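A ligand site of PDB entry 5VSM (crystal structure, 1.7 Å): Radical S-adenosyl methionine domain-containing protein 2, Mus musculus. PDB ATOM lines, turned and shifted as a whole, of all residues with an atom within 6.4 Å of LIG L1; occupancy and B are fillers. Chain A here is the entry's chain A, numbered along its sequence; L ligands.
The side-chain hydroxyl of Ser 113 sits at hydrogen-bond distance from the side-chain carboxylate of Glu 83 (2.7 Å). The guanidinium group of Arg 150 lies close to the side-chain sulfur of Cys 44 (3.7 Å). OG of Ser 113 sits at hydrogen-bond distance from N of Gly 115 (2.8 Å). N of Ser 136 is in hydrogen-bond range of O of Ser 113 (3.0 Å). The side-chain sulfur of Cys 47 sits close to the backbone carbonyl oxygen of His 49, at 3.4 Å. The side-chain carboxylate of Glu 83 lies within hydrogen-bond range of the backbone NH of Asn 114 (2.8 Å). The backbone carbonyl oxygen (O) of Gly 81 lies within hydrogen-bond range of a ring nitrogen (ND1) of His 35 (2.8 Å). O of Phe 79 lies within hydrogen-bond range of N of Val 112 (3.0 Å).
NH2 of Arg 150 is in hydrogen-bond range of O2 of LG3 L3, 2.8 Å away. The side-chain sulfur (SG) of Cys 40 is bound to an iron atom (FE1) of LG2 L2, 2.4 Å away. A sulfur (S2) of LG2 L2 lies close to the backbone NH (N) of Gly 82. A nitrogen (N1) of LIG L1 lies close to the side-chain carboxylate of Glu 83, at 3.5 Å. O of Gly 82 lies close to N1 of LIG L1 (2.9 Å). S4 of LG2 L2 sits close to N of Cys 44 (3.5 Å). An oxygen (O1) of LIG L1 lies close to the guanidinium group (NH1) of Arg 150 (2.9 Å). ND2 of Asn 114 sits close to S3 of LG2 L2. The backbone NH (N) of Phe 48 lies close to a nitrogen (N4) of LG3 L3, at 3.4 Å. O2 of LIG L1 is in hydrogen-bond range of OG of Ser 136 (2.4 Å). OG of Ser 136 is in hydrogen-bond range of O3 of LG3 L3, at 2.7 Å. SG of Cys 47 binds FE3 of LG2 L2 (2.4 Å). O3 of LG3 L3 sits at hydrogen-bond distance from ND2 of Asn 178, 3.1 Å away. S3 of LG2 L2 lies close to NH1 of Arg 150 (3.4 Å). SG of Cys 44 is bound to FE2 of LG2 L2 (2.4 Å).
O of Ser 113 sits close to O2 of LIG L1, 3.3 Å away. CB of His 49 touches C5 of LIG L1, at 3.8 Å. Ser 80 touches LIG L1. Gly 81 touches LIG L1 (O to C4, 3.4 Å). CG2 of Val 112 touches O2 of LIG L1 (3.4 Å). N of Asn 114 touches O2 of LIG L1 (3.5 Å). Hydrophobic or aromatic side chains that line LIG L1: His 49 and Val 112. Ten residues have an atom within 4 Å of LIG L1: His 49, Ser 80, Gly 81, Gly 82, Glu 83, Val 112, Ser 113, Asn 114, Ser 136 and Arg 150. Along chain A the residues within 4 Å of LIG L1 span positions 49 to 150. The nearest printed residue that does not touch LIG L1 is Phe 48 (4.002 Å).
An iron atom (FE4) of LG2 L2 is bound by an oxygen (O1) of LIG L1 (2.3 Å).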
ATOM      1  N   HIS A  35       3.874 -17.161  24.190  1.00  0.00           N
ATOM      2  CA  HIS A  35       3.262 -17.991  23.144  1.00  0.00           C
ATOM      3  C   HIS A  35       3.831 -17.538  21.809  1.00  0.00           C
ATOM      4  O   HIS A  35       3.222 -16.773  21.050  1.00  0.00           O
ATOM      5  CB  HIS A  35       1.738 -17.885  23.199  1.00  0.00           C
ATOM      6  CG  HIS A  35       1.144 -18.420  24.469  1.00  0.00           C
ATOM      7  ND1 HIS A  35       0.367 -19.557  24.507  1.00  0.00           N
ATOM      8  CD2 HIS A  35       1.233 -17.987  25.747  1.00  0.00           C
ATOM      9  CE1 HIS A  35       0.000 -19.805  25.753  1.00  0.00           C
ATOM     10  NE2 HIS A  35       0.508 -18.858  26.521  1.00  0.00           N
ATOM     11  N   CYS A  40       0.381 -25.664  15.356  1.00  0.00           N
ATOM     12  CA  CYS A  40       0.356 -26.875  16.169  1.00  0.00           C
ATOM     13  C   CYS A  40       0.011 -28.065  15.300  1.00  0.00           C
ATOM     14  O   CYS A  40      -0.672 -27.931  14.279  1.00  0.00           O
ATOM     15  CB  CYS A  40      -0.654 -26.771  17.316  1.00  0.00           C
ATOM     16  SG  CYS A  40      -0.512 -28.185  18.423  1.00  0.00           S
ATOM     17  N   TYR A  42      -1.517 -30.839  16.791  1.00  0.00           N
ATOM     18  CA  TYR A  42      -2.670 -31.474  17.421  1.00  0.00           C
ATOM     19  C   TYR A  42      -3.949 -30.719  17.073  1.00  0.00           C
ATOM     20  O   TYR A  42      -3.919 -29.660  16.437  1.00  0.00           O
ATOM     21  CB  TYR A  42      -2.496 -31.539  18.948  1.00  0.00           C
ATOM     22  CG  TYR A  42      -1.711 -32.727  19.480  1.00  0.00           C
ATOM     23  CD1 TYR A  42      -0.950 -33.544  18.633  1.00  0.00           C
ATOM     24  CD2 TYR A  42      -1.745 -33.032  20.836  1.00  0.00           C
ATOM     25  CE1 TYR A  42      -0.240 -34.635  19.149  1.00  0.00           C
ATOM     26  CE2 TYR A  42      -1.035 -34.112  21.351  1.00  0.00           C
ATOM     27  CZ  TYR A  42      -0.292 -34.907  20.511  1.00  0.00           C
ATOM     28  OH  TYR A  42       0.397 -35.986  21.020  1.00  0.00           O
ATOM     29  N   CYS A  44      -6.769 -30.278  19.565  1.00  0.00           N
ATOM     30  CA  CYS A  44      -7.576 -30.301  20.781  1.00  0.00           C
ATOM     31  C   CYS A  44      -8.823 -29.440  20.611  1.00  0.00           C
ATOM     32  O   CYS A  44      -8.737 -28.271  20.243  1.00  0.00           O
ATOM     33  CB  CYS A  44      -6.745 -29.817  21.971  1.00  0.00           C
ATOM     34  SG  CYS A  44      -5.175 -30.730  22.174  1.00  0.00           S
ATOM     35  N   CYS A  47      -8.903 -26.078  22.492  1.00  0.00           N
ATOM     36  CA  CYS A  47      -7.683 -25.268  22.445  1.00  0.00           C
ATOM     37  C   CYS A  47      -7.980 -23.772  22.565  1.00  0.00           C
ATOM     38  O   CYS A  47      -8.747 -23.224  21.775  1.00  0.00           O
ATOM     39  CB  CYS A  47      -6.931 -25.536  21.139  1.00  0.00           C
ATOM     40  SG  CYS A  47      -5.455 -24.485  20.992  1.00  0.00           S
ATOM     41  N   PHE A  48      -7.385 -23.093  23.563  1.00  0.00           N
ATOM     42  CA  PHE A  48      -7.688 -21.683  23.745  1.00  0.00           C
ATOM     43  C   PHE A  48      -6.600 -20.745  23.229  1.00  0.00           C
ATOM     44  O   PHE A  48      -6.687 -19.535  23.476  1.00  0.00           O
ATOM     45  CB  PHE A  48      -8.039 -21.367  25.210  1.00  0.00           C
ATOM     46  CG  PHE A  48      -6.917 -21.516  26.214  1.00  0.00           C
ATOM     47  CD1 PHE A  48      -7.149 -21.179  27.539  1.00  0.00           C
ATOM     48  CD2 PHE A  48      -5.661 -21.984  25.869  1.00  0.00           C
ATOM     49  CE1 PHE A  48      -6.154 -21.297  28.504  1.00  0.00           C
ATOM     50  CE2 PHE A  48      -4.660 -22.114  26.814  1.00  0.00           C
ATOM     51  CZ  PHE A  48      -4.906 -21.766  28.138  1.00  0.00           C
ATOM     52  N   HIS A  49      -5.625 -21.246  22.479  1.00  0.00           N
ATOM     53  CA  HIS A  49      -4.628 -20.396  21.822  1.00  0.00           C
ATOM     54  C   HIS A  49      -4.382 -21.000  20.440  1.00  0.00           C
ATOM     55  O   HIS A  49      -3.468 -21.797  20.253  1.00  0.00           O
ATOM     56  CB  HIS A  49      -3.344 -20.281  22.623  1.00  0.00           C
ATOM     57  CG  HIS A  49      -2.565 -19.038  22.309  1.00  0.00           C
ATOM     58  ND1 HIS A  49      -2.919 -17.807  22.814  1.00  0.00           N
ATOM     59  CD2 HIS A  49      -1.497 -18.827  21.512  1.00  0.00           C
ATOM     60  CE1 HIS A  49      -2.094 -16.890  22.345  1.00  0.00           C
ATOM     61  NE2 HIS A  49      -1.215 -17.484  21.561  1.00  0.00           N
ATOM     62  N   THR A  50      -5.227 -20.594  19.490  1.00  0.00           N
ATOM     63  CA  THR A  50      -5.437 -21.315  18.238  1.00  0.00           C
ATOM     64  C   THR A  50      -4.553 -20.781  17.113  1.00  0.00           C
ATOM     65  O   THR A  50      -3.896 -19.755  17.226  1.00  0.00           O
ATOM     66  CB  THR A  50      -6.915 -21.238  17.846  1.00  0.00           C
ATOM     67  OG1 THR A  50      -7.301 -19.872  17.630  1.00  0.00           O
ATOM     68  CG2 THR A  50      -7.764 -21.846  18.959  1.00  0.00           C
ATOM     69  N   PHE A  79       7.924 -20.968  27.785  1.00  0.00           N
ATOM     70  CA  PHE A  79       7.672 -21.001  26.337  1.00  0.00           C
ATOM     71  C   PHE A  79       6.462 -21.872  26.032  1.00  0.00           C
ATOM     72  O   PHE A  79       6.367 -23.015  26.498  1.00  0.00           O
ATOM     73  CB  PHE A  79       8.892 -21.537  25.600  1.00  0.00           C
ATOM     74  CG  PHE A  79      10.058 -20.587  25.619  1.00  0.00           C
ATOM     75  CD1 PHE A  79      10.181 -19.616  24.644  1.00  0.00           C
ATOM     76  CD2 PHE A  79      11.011 -20.648  26.633  1.00  0.00           C
ATOM     77  CE1 PHE A  79      11.248 -18.726  24.663  1.00  0.00           C
ATOM     78  CE2 PHE A  79      12.077 -19.768  26.652  1.00  0.00           C
ATOM     79  CZ  PHE A  79      12.192 -18.807  25.671  1.00  0.00           C
ATOM     80  N   SER A  80       5.558 -21.331  25.226  1.00  0.00           N
ATOM     81  CA  SER A  80       4.262 -21.949  24.969  1.00  0.00           C
ATOM     82  C   SER A  80       3.850 -21.664  23.518  1.00  0.00           C
ATOM     83  O   SER A  80       4.646 -21.185  22.704  1.00  0.00           O
ATOM     84  CB  SER A  80       3.218 -21.437  25.955  1.00  0.00           C
ATOM     85  OG  SER A  80       2.084 -22.290  25.937  1.00  0.00           O
ATOM     86  N   GLY A  81       2.588 -21.926  23.199  1.00  0.00           N
ATOM     87  CA  GLY A  81       2.107 -21.720  21.848  1.00  0.00           C
ATOM     88  C   GLY A  81       0.619 -21.969  21.714  1.00  0.00           C
ATOM     89  O   GLY A  81      -0.142 -21.573  22.596  1.00  0.00           O
ATOM     90  N   GLY A  82       0.172 -22.627  20.631  1.00  0.00           N
ATOM     91  CA  GLY A  82       1.037 -23.301  19.667  1.00  0.00           C
ATOM     92  C   GLY A  82       1.841 -24.467  20.254  1.00  0.00           C
ATOM     93  O   GLY A  82       1.905 -24.660  21.465  1.00  0.00           O
ATOM     94  N   GLU A  83       2.467 -25.272  19.391  1.00  0.00           N
ATOM     95  CA  GLU A  83       3.350 -26.322  19.869  1.00  0.00           C
ATOM     96  C   GLU A  83       4.786 -25.818  19.779  1.00  0.00           C
ATOM     97  O   GLU A  83       5.280 -25.617  18.658  1.00  0.00           O
ATOM     98  CB  GLU A  83       3.177 -27.587  19.047  1.00  0.00           C
ATOM     99  CG  GLU A  83       4.157 -28.694  19.404  1.00  0.00           C
ATOM    100  CD  GLU A  83       4.409 -28.819  20.888  1.00  0.00           C
ATOM    101  OE1 GLU A  83       3.443 -28.860  21.673  1.00  0.00           O
ATOM    102  OE2 GLU A  83       5.588 -28.897  21.292  1.00  0.00           O
ATOM    103  N   PRO A  84       5.469 -25.574  20.909  1.00  0.00           N
ATOM    104  CA  PRO A  84       6.822 -24.989  20.854  1.00  0.00           C
ATOM    105  C   PRO A  84       7.821 -25.789  20.033  1.00  0.00           C
ATOM    106  O   PRO A  84       8.715 -25.188  19.414  1.00  0.00           O
ATOM    107  CB  PRO A  84       7.241 -24.940  22.330  1.00  0.00           C
ATOM    108  CG  PRO A  84       5.937 -24.719  23.051  1.00  0.00           C
ATOM    109  CD  PRO A  84       4.947 -25.586  22.291  1.00  0.00           C
ATOM    110  N   VAL A 112       6.120 -25.628  27.943  1.00  0.00           N
ATOM    111  CA  VAL A 112       4.926 -26.462  27.990  1.00  0.00           C
ATOM    112  C   VAL A 112       4.667 -26.985  26.581  1.00  0.00           C
ATOM    113  O   VAL A 112       4.627 -26.218  25.623  1.00  0.00           O
ATOM    114  CB  VAL A 112       3.701 -25.703  28.553  1.00  0.00           C
ATOM    115  CG1 VAL A 112       3.476 -24.392  27.809  1.00  0.00           C
ATOM    116  CG2 VAL A 112       2.456 -26.577  28.491  1.00  0.00           C
ATOM    117  N   SER A 113       4.526 -28.307  26.455  1.00  0.00           N
ATOM    118  CA  SER A 113       4.493 -28.948  25.150  1.00  0.00           C
ATOM    119  C   SER A 113       3.486 -30.086  25.127  1.00  0.00           C
ATOM    120  O   SER A 113       3.222 -30.718  26.154  1.00  0.00           O
ATOM    121  CB  SER A 113       5.901 -29.462  24.801  1.00  0.00           C
ATOM    122  OG  SER A 113       5.883 -30.278  23.631  1.00  0.00           O
ATOM    123  N   ASN A 114       2.959 -30.389  23.930  1.00  0.00           N
ATOM    124  CA  ASN A 114       2.195 -31.625  23.846  1.00  0.00           C
ATOM    125  C   ASN A 114       3.090 -32.858  23.759  1.00  0.00           C
ATOM    126  O   ASN A 114       2.578 -33.980  23.822  1.00  0.00           O
ATOM    127  CB  ASN A 114       1.185 -31.586  22.687  1.00  0.00           C
ATOM    128  CG  ASN A 114       1.822 -31.627  21.282  1.00  0.00           C
ATOM    129  OD1 ASN A 114       2.876 -32.219  21.043  1.00  0.00           O
ATOM    130  ND2 ASN A 114       1.102 -31.033  20.310  1.00  0.00           N
ATOM    131  N   GLY A 115       4.406 -32.676  23.634  1.00  0.00           N
ATOM    132  CA  GLY A 115       5.357 -33.762  23.743  1.00  0.00           C
ATOM    133  C   GLY A 115       5.585 -34.579  22.485  1.00  0.00           C
ATOM    134  O   GLY A 115       6.647 -35.206  22.354  1.00  0.00           O
ATOM    135  N   ALA A 134       6.940 -29.171  30.952  1.00  0.00           N
ATOM    136  CA  ALA A 134       5.584 -29.557  31.330  1.00  0.00           C
ATOM    137  C   ALA A 134       4.932 -30.153  30.089  1.00  0.00           C
ATOM    138  O   ALA A 134       4.904 -29.513  29.038  1.00  0.00           O
ATOM    139  CB  ALA A 134       4.772 -28.360  31.840  1.00  0.00           C
ATOM    140  N   ILE A 135       4.460 -31.387  30.206  1.00  0.00           N
ATOM    141  CA  ILE A 135       3.811 -32.076  29.104  1.00  0.00           C
ATOM    142  C   ILE A 135       2.311 -32.090  29.392  1.00  0.00           C
ATOM    143  O   ILE A 135       1.884 -32.460  30.490  1.00  0.00           O
ATOM    144  CB  ILE A 135       4.332 -33.507  28.922  1.00  0.00           C
ATOM    145  CG1 ILE A 135       5.852 -33.523  28.685  1.00  0.00           C
ATOM    146  CG2 ILE A 135       3.632 -34.176  27.730  1.00  0.00           C
ATOM    147  CD1 ILE A 135       6.273 -32.642  27.533  1.00  0.00           C
ATOM    148  N   SER A 136       1.526 -31.713  28.391  1.00  0.00           N
ATOM    149  CA  SER A 136       0.070 -31.660  28.503  1.00  0.00           C
ATOM    150  C   SER A 136      -0.522 -33.035  28.227  1.00  0.00           C
ATOM    151  O   SER A 136      -0.319 -33.597  27.142  1.00  0.00           O
ATOM    152  CB  SER A 136      -0.483 -30.630  27.537  1.00  0.00           C
ATOM    153  OG  SER A 136      -0.114 -29.317  27.945  1.00  0.00           O
ATOM    154  N   ARG A 150      -6.316 -34.548  21.300  1.00  0.00           N
ATOM    155  CA  ARG A 150      -4.969 -34.502  21.867  1.00  0.00           C
ATOM    156  C   ARG A 150      -4.186 -35.662  21.243  1.00  0.00           C
ATOM    157  O   ARG A 150      -3.885 -36.685  21.864  1.00  0.00           O
ATOM    158  CB  ARG A 150      -5.039 -34.583  23.391  1.00  0.00           C
ATOM    159  CG  ARG A 150      -3.689 -34.498  24.119  1.00  0.00           C
ATOM    160  CD  ARG A 150      -3.156 -33.079  24.196  1.00  0.00           C
ATOM    161  NE  ARG A 150      -3.828 -32.281  25.210  1.00  0.00           N
ATOM    162  CZ  ARG A 150      -3.510 -31.019  25.495  1.00  0.00           C
ATOM    163  NH1 ARG A 150      -2.540 -30.419  24.824  1.00  0.00           N
ATOM    164  NH2 ARG A 150      -4.156 -30.359  26.444  1.00  0.00           N
ATOM    165  N   ASN A 178       0.527 -31.160  32.810  1.00  0.00           N
ATOM    166  CA  ASN A 178      -0.619 -30.251  32.767  1.00  0.00           C
ATOM    167  C   ASN A 178      -1.815 -31.045  32.231  1.00  0.00           C
ATOM    168  O   ASN A 178      -1.682 -31.776  31.257  1.00  0.00           O
ATOM    169  CB  ASN A 178      -0.408 -29.065  31.827  1.00  0.00           C
ATOM    170  CG  ASN A 178       0.650 -28.069  32.316  1.00  0.00           C
ATOM    171  OD1 ASN A 178       1.299 -28.259  33.355  1.00  0.00           O
ATOM    172  ND2 ASN A 178       0.807 -26.987  31.575  1.00  0.00           N
HETATM  173  N1  LIG L   1       0.691 -26.925  22.705  1.00  0.00           N
HETATM  174  C1  LIG L   1       1.217 -26.904  24.079  1.00  0.00           C
HETATM  175  C2  LIG L   1       0.389 -27.841  24.932  1.00  0.00           C
HETATM  176  O1  LIG L   1      -0.761 -28.151  24.681  1.00  0.00           O
HETATM  177  C3  LIG L   1       1.234 -25.502  24.709  1.00  0.00           C
HETATM  178  C4  LIG L   1       0.172 -24.527  24.199  1.00  0.00           C
HETATM  179  S1  LIG L   1      -1.501 -25.090  24.613  1.00  0.00           S
HETATM  180  C5  LIG L   1      -2.506 -23.761  23.870  1.00  0.00           C
HETATM  181  O2  LIG L   1       0.943 -28.351  26.012  1.00  0.00           O
HETATM  182 FE1  LG2 L   2      -2.046 -27.704  20.140  1.00  0.00          FE
HETATM  183 FE2  LG2 L   2      -3.744 -28.871  21.811  1.00  0.00          FE
HETATM  184 FE3  LG2 L   2      -3.874 -26.246  21.358  1.00  0.00          FE
HETATM  185 FE4  LG2 L   2      -1.655 -27.164  22.832  1.00  0.00          FE
HETATM  186  S1  LG2 L   2      -4.003 -27.271  23.349  1.00  0.00           S
HETATM  187  S2  LG2 L   2      -1.745 -25.687  20.968  1.00  0.00           S
HETATM  188  S3  LG2 L   2      -1.544 -29.318  21.760  1.00  0.00           S
HETATM  189  S4  LG2 L   2      -4.254 -27.902  19.812  1.00  0.00           S
HETATM  190  N1  LG3 L   3      -8.601 -24.242  29.034  1.00  0.00           N
HETATM  191  C1  LG3 L   3      -7.629 -24.424  29.904  1.00  0.00           C
HETATM  192  N2  LG3 L   3      -6.425 -24.837  29.544  1.00  0.00           N
HETATM  193  C2  LG3 L   3      -6.151 -25.065  28.269  1.00  0.00           C
HETATM  194  N3  LG3 L   3      -5.045 -25.494  27.616  1.00  0.00           N
HETATM  195  C3  LG3 L   3      -5.332 -25.558  26.277  1.00  0.00           C
HETATM  196  N4  LG3 L   3      -6.591 -25.211  26.076  1.00  0.00           N
HETATM  197  C4  LG3 L   3      -7.149 -24.896  27.294  1.00  0.00           C
HETATM  198  C5  LG3 L   3      -8.405 -24.454  27.726  1.00  0.00           C
HETATM  199  N5  LG3 L   3      -9.429 -24.281  26.794  1.00  0.00           N
HETATM  200  C6  LG3 L   3      -3.783 -25.775  28.317  1.00  0.00           C
HETATM  201  C7  LG3 L   3      -2.798 -26.634  27.492  1.00  0.00           C
HETATM  202  C8  LG3 L   3      -1.452 -26.308  28.208  1.00  0.00           C
HETATM  203  C9  LG3 L   3      -1.714 -24.919  28.829  1.00  0.00           C
HETATM  204  C10 LG3 L   3      -0.774 -23.870  28.214  1.00  0.00           C
HETATM  205  O1  LG3 L   3      -3.055 -24.543  28.438  1.00  0.00           O
HETATM  206  O2  LG3 L   3      -3.164 -28.012  27.576  1.00  0.00           O
HETATM  207  O3  LG3 L   3      -1.200 -27.253  29.252  1.00  0.00           O
